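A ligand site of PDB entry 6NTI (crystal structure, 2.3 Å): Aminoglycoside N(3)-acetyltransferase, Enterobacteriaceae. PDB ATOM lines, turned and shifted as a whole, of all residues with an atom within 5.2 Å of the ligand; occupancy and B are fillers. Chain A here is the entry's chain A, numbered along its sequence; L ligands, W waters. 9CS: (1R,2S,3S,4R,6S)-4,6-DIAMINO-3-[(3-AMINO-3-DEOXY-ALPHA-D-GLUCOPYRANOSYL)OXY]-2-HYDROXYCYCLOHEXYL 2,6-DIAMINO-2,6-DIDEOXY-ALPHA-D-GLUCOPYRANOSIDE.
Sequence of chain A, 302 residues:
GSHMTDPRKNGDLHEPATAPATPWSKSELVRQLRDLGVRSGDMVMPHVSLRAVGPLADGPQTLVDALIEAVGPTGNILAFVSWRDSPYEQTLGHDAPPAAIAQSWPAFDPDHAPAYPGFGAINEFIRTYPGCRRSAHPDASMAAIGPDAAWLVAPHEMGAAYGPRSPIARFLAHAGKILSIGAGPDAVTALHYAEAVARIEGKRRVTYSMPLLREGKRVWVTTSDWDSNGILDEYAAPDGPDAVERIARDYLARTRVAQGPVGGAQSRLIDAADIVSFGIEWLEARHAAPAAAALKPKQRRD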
ATOM      1  N   PHE A  80      34.159  21.151  20.434  1.00  0.00           N
ATOM      2  CA  PHE A  80      32.932  20.804  21.154  1.00  0.00           C
ATOM      3  C   PHE A  80      31.761  21.107  20.223  1.00  0.00           C
ATOM      4  O   PHE A  80      31.372  22.264  20.042  1.00  0.00           O
ATOM      5  CB  PHE A  80      32.847  21.595  22.460  1.00  0.00           C
ATOM      6  CG  PHE A  80      31.539  21.457  23.180  1.00  0.00           C
ATOM      7  CD1 PHE A  80      30.901  22.573  23.705  1.00  0.00           C
ATOM      8  CD2 PHE A  80      30.946  20.214  23.352  1.00  0.00           C
ATOM      9  CE1 PHE A  80      29.707  22.455  24.380  1.00  0.00           C
ATOM     10  CE2 PHE A  80      29.740  20.087  24.029  1.00  0.00           C
ATOM     11  CZ  PHE A  80      29.119  21.214  24.545  1.00  0.00           C
ATOM     12  N   SER A  82      28.637  19.035  20.138  1.00  0.00           N
ATOM     13  CA  SER A  82      27.356  18.655  20.735  1.00  0.00           C
ATOM     14  C   SER A  82      26.431  18.118  19.638  1.00  0.00           C
ATOM     15  O   SER A  82      26.892  17.483  18.674  1.00  0.00           O
ATOM     16  CB  SER A  82      26.799  19.819  21.517  1.00  0.00           C
ATOM     17  OG  SER A  82      25.617  19.445  22.215  1.00  0.00           O
ATOM     18  N   SER A  86      19.641  17.560  20.603  1.00  0.00           N
ATOM     19  CA  SER A  86      19.779  16.949  21.920  1.00  0.00           C
ATOM     20  C   SER A  86      18.512  17.166  22.733  1.00  0.00           C
ATOM     21  O   SER A  86      18.072  18.312  22.896  1.00  0.00           O
ATOM     22  CB  SER A  86      20.988  17.532  22.654  1.00  0.00           C
ATOM     23  OG  SER A  86      21.126  16.962  23.941  1.00  0.00           O
ATOM     24  N   TYR A  88      17.947  17.504  25.754  1.00  0.00           N
ATOM     25  CA  TYR A  88      18.423  17.818  27.104  1.00  0.00           C
ATOM     26  C   TYR A  88      17.312  18.420  27.955  1.00  0.00           C
ATOM     27  O   TYR A  88      16.978  17.906  29.025  1.00  0.00           O
ATOM     28  CB  TYR A  88      19.627  18.759  27.026  1.00  0.00           C
ATOM     29  CG  TYR A  88      20.261  19.086  28.354  1.00  0.00           C
ATOM     30  CD1 TYR A  88      21.153  18.215  28.955  1.00  0.00           C
ATOM     31  CD2 TYR A  88      19.953  20.269  29.019  1.00  0.00           C
ATOM     32  CE1 TYR A  88      21.736  18.520  30.178  1.00  0.00           C
ATOM     33  CE2 TYR A  88      20.519  20.581  30.230  1.00  0.00           C
ATOM     34  CZ  TYR A  88      21.414  19.701  30.804  1.00  0.00           C
ATOM     35  OH  TYR A  88      21.986  20.006  32.018  1.00  0.00           O
ATOM     36  N   GLU A  89      16.719  19.522  27.487  1.00  0.00           N
ATOM     37  CA  GLU A  89      15.650  20.168  28.238  1.00  0.00           C
ATOM     38  C   GLU A  89      14.433  19.262  28.354  1.00  0.00           C
ATOM     39  O   GLU A  89      13.739  19.259  29.388  1.00  0.00           O
ATOM     40  CB  GLU A  89      15.259  21.498  27.589  1.00  0.00           C
ATOM     41  CG  GLU A  89      16.347  22.543  27.589  1.00  0.00           C
ATOM     42  CD  GLU A  89      17.183  22.531  26.323  1.00  0.00           C
ATOM     43  OE1 GLU A  89      17.814  23.564  26.017  1.00  0.00           O
ATOM     44  OE2 GLU A  89      17.196  21.489  25.630  1.00  0.00           O
ATOM     45  N   TYR A 116      25.523  21.268  17.135  1.00  0.00           N
ATOM     46  CA  TYR A 116      24.661  22.287  17.709  1.00  0.00           C
ATOM     47  C   TYR A 116      25.086  23.661  17.197  1.00  0.00           C
ATOM     48  O   TYR A 116      26.237  24.062  17.399  1.00  0.00           O
ATOM     49  CB  TYR A 116      24.723  22.259  19.228  1.00  0.00           C
ATOM     50  CG  TYR A 116      23.721  23.165  19.905  1.00  0.00           C
ATOM     51  CD1 TYR A 116      22.370  22.844  19.944  1.00  0.00           C
ATOM     52  CD2 TYR A 116      24.129  24.345  20.515  1.00  0.00           C
ATOM     53  CE1 TYR A 116      21.450  23.668  20.562  1.00  0.00           C
ATOM     54  CE2 TYR A 116      23.221  25.178  21.132  1.00  0.00           C
ATOM     55  CZ  TYR A 116      21.890  24.840  21.157  1.00  0.00           C
ATOM     56  OH  TYR A 116      20.975  25.671  21.781  1.00  0.00           O
ATOM     57  N   PHE A 119      26.808  26.711  19.579  1.00  0.00           N
ATOM     58  CA  PHE A 119      28.195  26.715  20.025  1.00  0.00           C
ATOM     59  C   PHE A 119      29.162  27.141  18.926  1.00  0.00           C
ATOM     60  O   PHE A 119      30.373  27.010  19.101  1.00  0.00           O
ATOM     61  CB  PHE A 119      28.574  25.320  20.551  1.00  0.00           C
ATOM     62  CG  PHE A 119      27.727  24.854  21.703  1.00  0.00           C
ATOM     63  CD1 PHE A 119      27.201  25.767  22.606  1.00  0.00           C
ATOM     64  CD2 PHE A 119      27.455  23.513  21.883  1.00  0.00           C
ATOM     65  CE1 PHE A 119      26.430  25.339  23.671  1.00  0.00           C
ATOM     66  CE2 PHE A 119      26.673  23.085  22.939  1.00  0.00           C
ATOM     67  CZ  PHE A 119      26.166  23.995  23.831  1.00  0.00           C
ATOM     68  N   ASP A 139      25.038  14.602  24.046  1.00  0.00           N
ATOM     69  CA  ASP A 139      24.901  16.012  24.436  1.00  0.00           C
ATOM     70  C   ASP A 139      26.239  16.735  24.482  1.00  0.00           C
ATOM     71  O   ASP A 139      26.303  17.925  24.176  1.00  0.00           O
ATOM     72  CB  ASP A 139      24.212  16.108  25.798  1.00  0.00           C
ATOM     73  CG  ASP A 139      23.867  17.538  26.161  1.00  0.00           C
ATOM     74  OD1 ASP A 139      22.982  18.115  25.512  1.00  0.00           O
ATOM     75  OD2 ASP A 139      24.494  18.081  27.096  1.00  0.00           O
ATOM     76  N   TYR A 162      32.320  16.190  30.896  1.00  0.00           N
ATOM     77  CA  TYR A 162      33.508  17.027  30.830  1.00  0.00           C
ATOM     78  C   TYR A 162      34.539  16.697  31.903  1.00  0.00           C
ATOM     79  O   TYR A 162      35.601  17.321  31.939  1.00  0.00           O
ATOM     80  CB  TYR A 162      33.122  18.508  30.929  1.00  0.00           C
ATOM     81  CG  TYR A 162      31.941  18.866  30.046  1.00  0.00           C
ATOM     82  CD1 TYR A 162      30.656  18.905  30.565  1.00  0.00           C
ATOM     83  CD2 TYR A 162      32.124  19.155  28.703  1.00  0.00           C
ATOM     84  CE1 TYR A 162      29.577  19.226  29.745  1.00  0.00           C
ATOM     85  CE2 TYR A 162      31.069  19.470  27.888  1.00  0.00           C
ATOM     86  CZ  TYR A 162      29.794  19.508  28.416  1.00  0.00           C
ATOM     87  OH  TYR A 162      28.732  19.830  27.599  1.00  0.00           O
ATOM     88  N   ASP A 186      33.022  33.288  28.291  1.00  0.00           N
ATOM     89  CA  ASP A 186      32.064  32.259  28.665  1.00  0.00           C
ATOM     90  C   ASP A 186      32.193  30.988  27.834  1.00  0.00           C
ATOM     91  O   ASP A 186      31.528  30.000  28.149  1.00  0.00           O
ATOM     92  CB  ASP A 186      30.644  32.806  28.545  1.00  0.00           C
ATOM     93  CG  ASP A 186      30.341  33.313  27.152  1.00  0.00           C
ATOM     94  OD1 ASP A 186      31.147  34.091  26.604  1.00  0.00           O
ATOM     95  OD2 ASP A 186      29.289  32.931  26.595  1.00  0.00           O
ATOM     96  N   HIS A 192      34.817  23.441  32.413  1.00  0.00           N
ATOM     97  CA  HIS A 192      33.866  22.543  33.059  1.00  0.00           C
ATOM     98  C   HIS A 192      34.571  21.364  33.697  1.00  0.00           C
ATOM     99  O   HIS A 192      34.043  20.752  34.639  1.00  0.00           O
ATOM    100  CB  HIS A 192      32.815  22.069  32.059  1.00  0.00           C
ATOM    101  CG  HIS A 192      31.871  23.151  31.619  1.00  0.00           C
ATOM    102  ND1 HIS A 192      31.096  23.861  32.508  1.00  0.00           N
ATOM    103  CD2 HIS A 192      31.593  23.645  30.393  1.00  0.00           C
ATOM    104  CE1 HIS A 192      30.373  24.747  31.841  1.00  0.00           C
ATOM    105  NE2 HIS A 192      30.659  24.637  30.559  1.00  0.00           N
ATOM    106  N   SER A 228      26.296  21.525  34.005  1.00  0.00           N
ATOM    107  CA  SER A 228      27.174  22.342  33.167  1.00  0.00           C
ATOM    108  C   SER A 228      26.629  23.750  32.945  1.00  0.00           C
ATOM    109  O   SER A 228      27.241  24.517  32.187  1.00  0.00           O
ATOM    110  CB  SER A 228      27.406  21.654  31.814  1.00  0.00           C
ATOM    111  OG  SER A 228      26.203  21.549  31.081  1.00  0.00           O
ATOM    112  N   ASN A 229      25.427  24.165  33.586  1.00  0.00           N
ATOM    113  CA  ASN A 229      24.889  25.519  33.505  1.00  0.00           C
ATOM    114  C   ASN A 229      25.028  26.290  34.810  1.00  0.00           C
ATOM    115  O   ASN A 229      24.526  27.412  34.912  1.00  0.00           O
ATOM    116  CB  ASN A 229      23.430  25.479  33.055  1.00  0.00           C
ATOM    117  CG  ASN A 229      23.284  25.038  31.605  1.00  0.00           C
ATOM    118  OD1 ASN A 229      23.798  25.698  30.704  1.00  0.00           O
ATOM    119  ND2 ASN A 229      22.598  23.924  31.381  1.00  0.00           N
ATOM    120  N   GLY A 230      25.712  25.705  35.782  1.00  0.00           N
ATOM    121  CA  GLY A 230      26.118  26.416  36.976  1.00  0.00           C
ATOM    122  C   GLY A 230      26.426  25.395  38.057  1.00  0.00           C
ATOM    123  O   GLY A 230      25.518  24.697  38.512  1.00  0.00           O
ATOM    124  N   TYR A 235      26.088  30.616  40.440  1.00  0.00           N
ATOM    125  CA  TYR A 235      26.511  30.622  39.038  1.00  0.00           C
ATOM    126  C   TYR A 235      25.446  30.084  38.104  1.00  0.00           C
ATOM    127  O   TYR A 235      25.637  30.142  36.880  1.00  0.00           O
ATOM    128  CB  TYR A 235      27.801  29.810  38.879  1.00  0.00           C
ATOM    129  CG  TYR A 235      28.899  30.185  39.852  1.00  0.00           C
ATOM    130  CD1 TYR A 235      29.411  29.250  40.741  1.00  0.00           C
ATOM    131  CD2 TYR A 235      29.402  31.479  39.899  1.00  0.00           C
ATOM    132  CE1 TYR A 235      30.404  29.585  41.638  1.00  0.00           C
ATOM    133  CE2 TYR A 235      30.394  31.823  40.785  1.00  0.00           C
ATOM    134  CZ  TYR A 235      30.891  30.882  41.660  1.00  0.00           C
ATOM    135  OH  TYR A 235      31.890  31.220  42.549  1.00  0.00           O
ATOM    136  N   GLY A 240      23.700  36.809  34.560  1.00  0.00           N
ATOM    137  CA  GLY A 240      23.838  35.408  34.943  1.00  0.00           C
ATOM    138  C   GLY A 240      25.188  34.791  34.619  1.00  0.00           C
ATOM    139  O   GLY A 240      25.239  33.701  34.053  1.00  0.00           O
ATOM    140  N   ASP A 242      28.306  32.609  34.761  1.00  0.00           N
ATOM    141  CA  ASP A 242      28.595  31.354  35.424  1.00  0.00           C
ATOM    142  C   ASP A 242      30.027  31.348  35.946  1.00  0.00           C
ATOM    143  O   ASP A 242      30.768  32.317  35.813  1.00  0.00           O
ATOM    144  CB  ASP A 242      28.337  30.177  34.485  1.00  0.00           C
ATOM    145  CG  ASP A 242      29.254  30.172  33.265  1.00  0.00           C
ATOM    146  OD1 ASP A 242      29.938  31.192  33.017  1.00  0.00           O
ATOM    147  OD2 ASP A 242      29.286  29.150  32.553  1.00  0.00           O
ATOM    148  N   GLU A 245      32.798  31.858  33.095  1.00  0.00           N
ATOM    149  CA  GLU A 245      33.091  33.231  32.672  1.00  0.00           C
ATOM    150  C   GLU A 245      33.867  33.989  33.741  1.00  0.00           C
ATOM    151  O   GLU A 245      34.798  34.739  33.415  1.00  0.00           O
ATOM    152  CB  GLU A 245      31.794  33.962  32.331  1.00  0.00           C
ATOM    153  CG  GLU A 245      32.013  35.387  31.857  1.00  0.00           C
ATOM    154  CD  GLU A 245      30.732  36.067  31.407  1.00  0.00           C
ATOM    155  OE1 GLU A 245      30.748  37.292  31.203  1.00  0.00           O
ATOM    156  OE2 GLU A 245      29.712  35.369  31.251  1.00  0.00           O
HETATM  157  C1  9CS L   1      25.607  28.337  27.915  1.00  0.00           C
HETATM  158  C2  9CS L   1      25.967  29.572  27.067  1.00  0.00           C
HETATM  159  C3  9CS L   1      27.027  30.373  27.826  1.00  0.00           C
HETATM  160  C4  9CS L   1      26.568  30.716  29.238  1.00  0.00           C
HETATM  161  C5  9CS L   1      26.089  29.469  30.007  1.00  0.00           C
HETATM  162  C6  9CS L   1      25.457  29.889  31.332  1.00  0.00           C
HETATM  163  C7  9CS L   1      27.063  23.447  27.821  1.00  0.00           C
HETATM  164  C8  9CS L   1      25.635  23.916  28.118  1.00  0.00           C
HETATM  165  C9  9CS L   1      25.576  25.402  27.746  1.00  0.00           C
HETATM  166  C10 9CS L   1      26.615  26.172  28.505  1.00  0.00           C
HETATM  167  C11 9CS L   1      28.043  25.562  28.385  1.00  0.00           C
HETATM  168  C12 9CS L   1      28.063  24.114  28.762  1.00  0.00           C
HETATM  169  C13 9CS L   1      23.704  22.372  27.954  1.00  0.00           C
HETATM  170  C14 9CS L   1      23.356  21.270  26.918  1.00  0.00           C
HETATM  171  C15 9CS L   1      22.468  21.833  25.791  1.00  0.00           C
HETATM  172  C16 9CS L   1      21.225  22.554  26.358  1.00  0.00           C
HETATM  173  C17 9CS L   1      21.736  23.668  27.268  1.00  0.00           C
HETATM  174  C18 9CS L   1      20.641  24.516  27.930  1.00  0.00           C
HETATM  175  N1  9CS L   1      24.810  28.745  31.998  1.00  0.00           N
HETATM  176  N2  9CS L   1      28.781  26.486  29.278  1.00  0.00           N
HETATM  177  N3  9CS L   1      26.991  22.002  28.011  1.00  0.00           N
HETATM  178  N4  9CS L   1      22.108  20.745  24.869  1.00  0.00           N
HETATM  179  O5  9CS L   1      25.134  28.789  29.197  1.00  0.00           O
HETATM  180  O7  9CS L   1      27.278  31.597  27.095  1.00  0.00           O
HETATM  181  O8  9CS L   1      27.688  31.261  29.966  1.00  0.00           O
HETATM  182  O9  9CS L   1      26.773  27.529  28.055  1.00  0.00           O
HETATM  183  O10 9CS L   1      24.257  25.836  28.100  1.00  0.00           O
HETATM  184  O11 9CS L   1      24.668  23.232  27.323  1.00  0.00           O
HETATM  185  O12 9CS L   1      22.533  23.102  28.316  1.00  0.00           O
HETATM  186  O13 9CS L   1      24.602  20.829  26.323  1.00  0.00           O
HETATM  187  O14 9CS L   1      20.491  23.113  25.267  1.00  0.00           O
HETATM  188  O15 9CS L   1      19.763  23.718  28.748  1.00  0.00           O
HETATM  189  N6  9CS L   1      26.519  29.176  25.761  1.00  0.00           N
HETATM  190  O   HOH W   1      28.081  33.321  31.641  1.00  0.00           O
HETATM  191  O   HOH W   2      27.459  27.247  31.774  1.00  0.00           O
HETATM  192  O   HOH W   3      30.990  27.443  27.955  1.00  0.00           O
HETATM  193  O   HOH W   4      29.793  29.072  30.053  1.00  0.00           O
HETATM  194  O   HOH W   5      24.558  30.615  34.333  1.00  0.00           O
HETATM  195  O   HOH W   6      22.912  27.740  25.836  1.00  0.00           O
HETATM  196  O   HOH W   7      19.384  20.913  24.029  1.00  0.00           O
HETATM  197  O   HOH W   8      23.482  21.341  22.724  1.00  0.00           O
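An oxygen (O7) of the ligand sits at hydrogen-bond distance from the side-chain carboxylate (OD2) of Asp 186. A nitrogen (N2) of the ligand lies within hydrogen-bond range of a ring nitrogen (NE2) of His 192 (2.9 Å). An oxygen (O14) of the ligand sits at hydrogen-bond distance from the side-chain carboxylate (OE1) of Glu 89, at 2.8 Å. The side-chain carboxylate of Asp 139 lies within salt-bridge range of a nitrogen (N4) of the ligand (2.8 Å). The backbone carbonyl oxygen of Asn 229 lies within hydrogen-bond range of a nitrogen (N1) of the ligand (3.2 Å). The side-chain hydroxyl of Tyr 162 sits at hydrogen-bond distance from a nitrogen (N3) of the ligand (2.8 Å). The side-chain hydroxyl (OG) of Ser 228 lies within hydrogen-bond range of a nitrogen (N3) of the ligand. O10 of the ligand sits at hydrogen-bond distance from OD1 of Asn 229 (2.6 Å).
OD1 of Asp 242 lies within hydrogen-bond range of N of Glu 245 (2.9 Å). The backbone carbonyl oxygen (O) of Asp 139 lies within hydrogen-bond range of the side-chain hydroxyl (OG) of Ser 82, 2.6 Å away. The side-chain carboxylate (OD1) of Asp 139 sits at hydrogen-bond distance from the side-chain hydroxyl (OG) of Ser 86 (2.7 Å).
Tyr 88 touches the ligand (CD2 to O15, 3.5 Å). CZ of Phe 119 touches O11 of the ligand, at 3.9 Å. OD2 of Asp 242 touches O8 of the ligand, 3.7 Å away. Hydrophobic or aromatic side chains that line the ligand: Tyr 88, Phe 119, Tyr 162 and His 192. The nearest printed residue that does not touch the ligand is Ser 86 (4.02 Å).
Water W8 lies within hydrogen-bond range of N4 of the ligand and OG of Ser 82. Water W1 lies within hydrogen-bond range of the side-chain carboxylate of Glu 245 (2.6 Å), an oxygen (O8) of the ligand (2.7 Å) and the side-chain carboxylate of Asp 242 (3.1 Å). Water W3 lies within hydrogen-bond range of O of Asp 186 (2.6 Å) and N2 of the ligand (2.7 Å). Water W7 lies within hydrogen-bond range of O14 of the ligand, OE2 of Glu 89 and O of Ser 86. Water W4 lies within hydrogen-bond range of the side-chain carboxylate (OD2) of Asp 242 (2.6 Å), the backbone carbonyl oxygen (O) of Asp 186 (2.7 Å) and a nitrogen (N2) of the ligand (2.9 Å). Water W2 lies within hydrogen-bond range of OD2 of Asp 242 (2.8 Å), O of Ser 228 (2.8 Å) and N2 of the ligand (2.9 Å).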
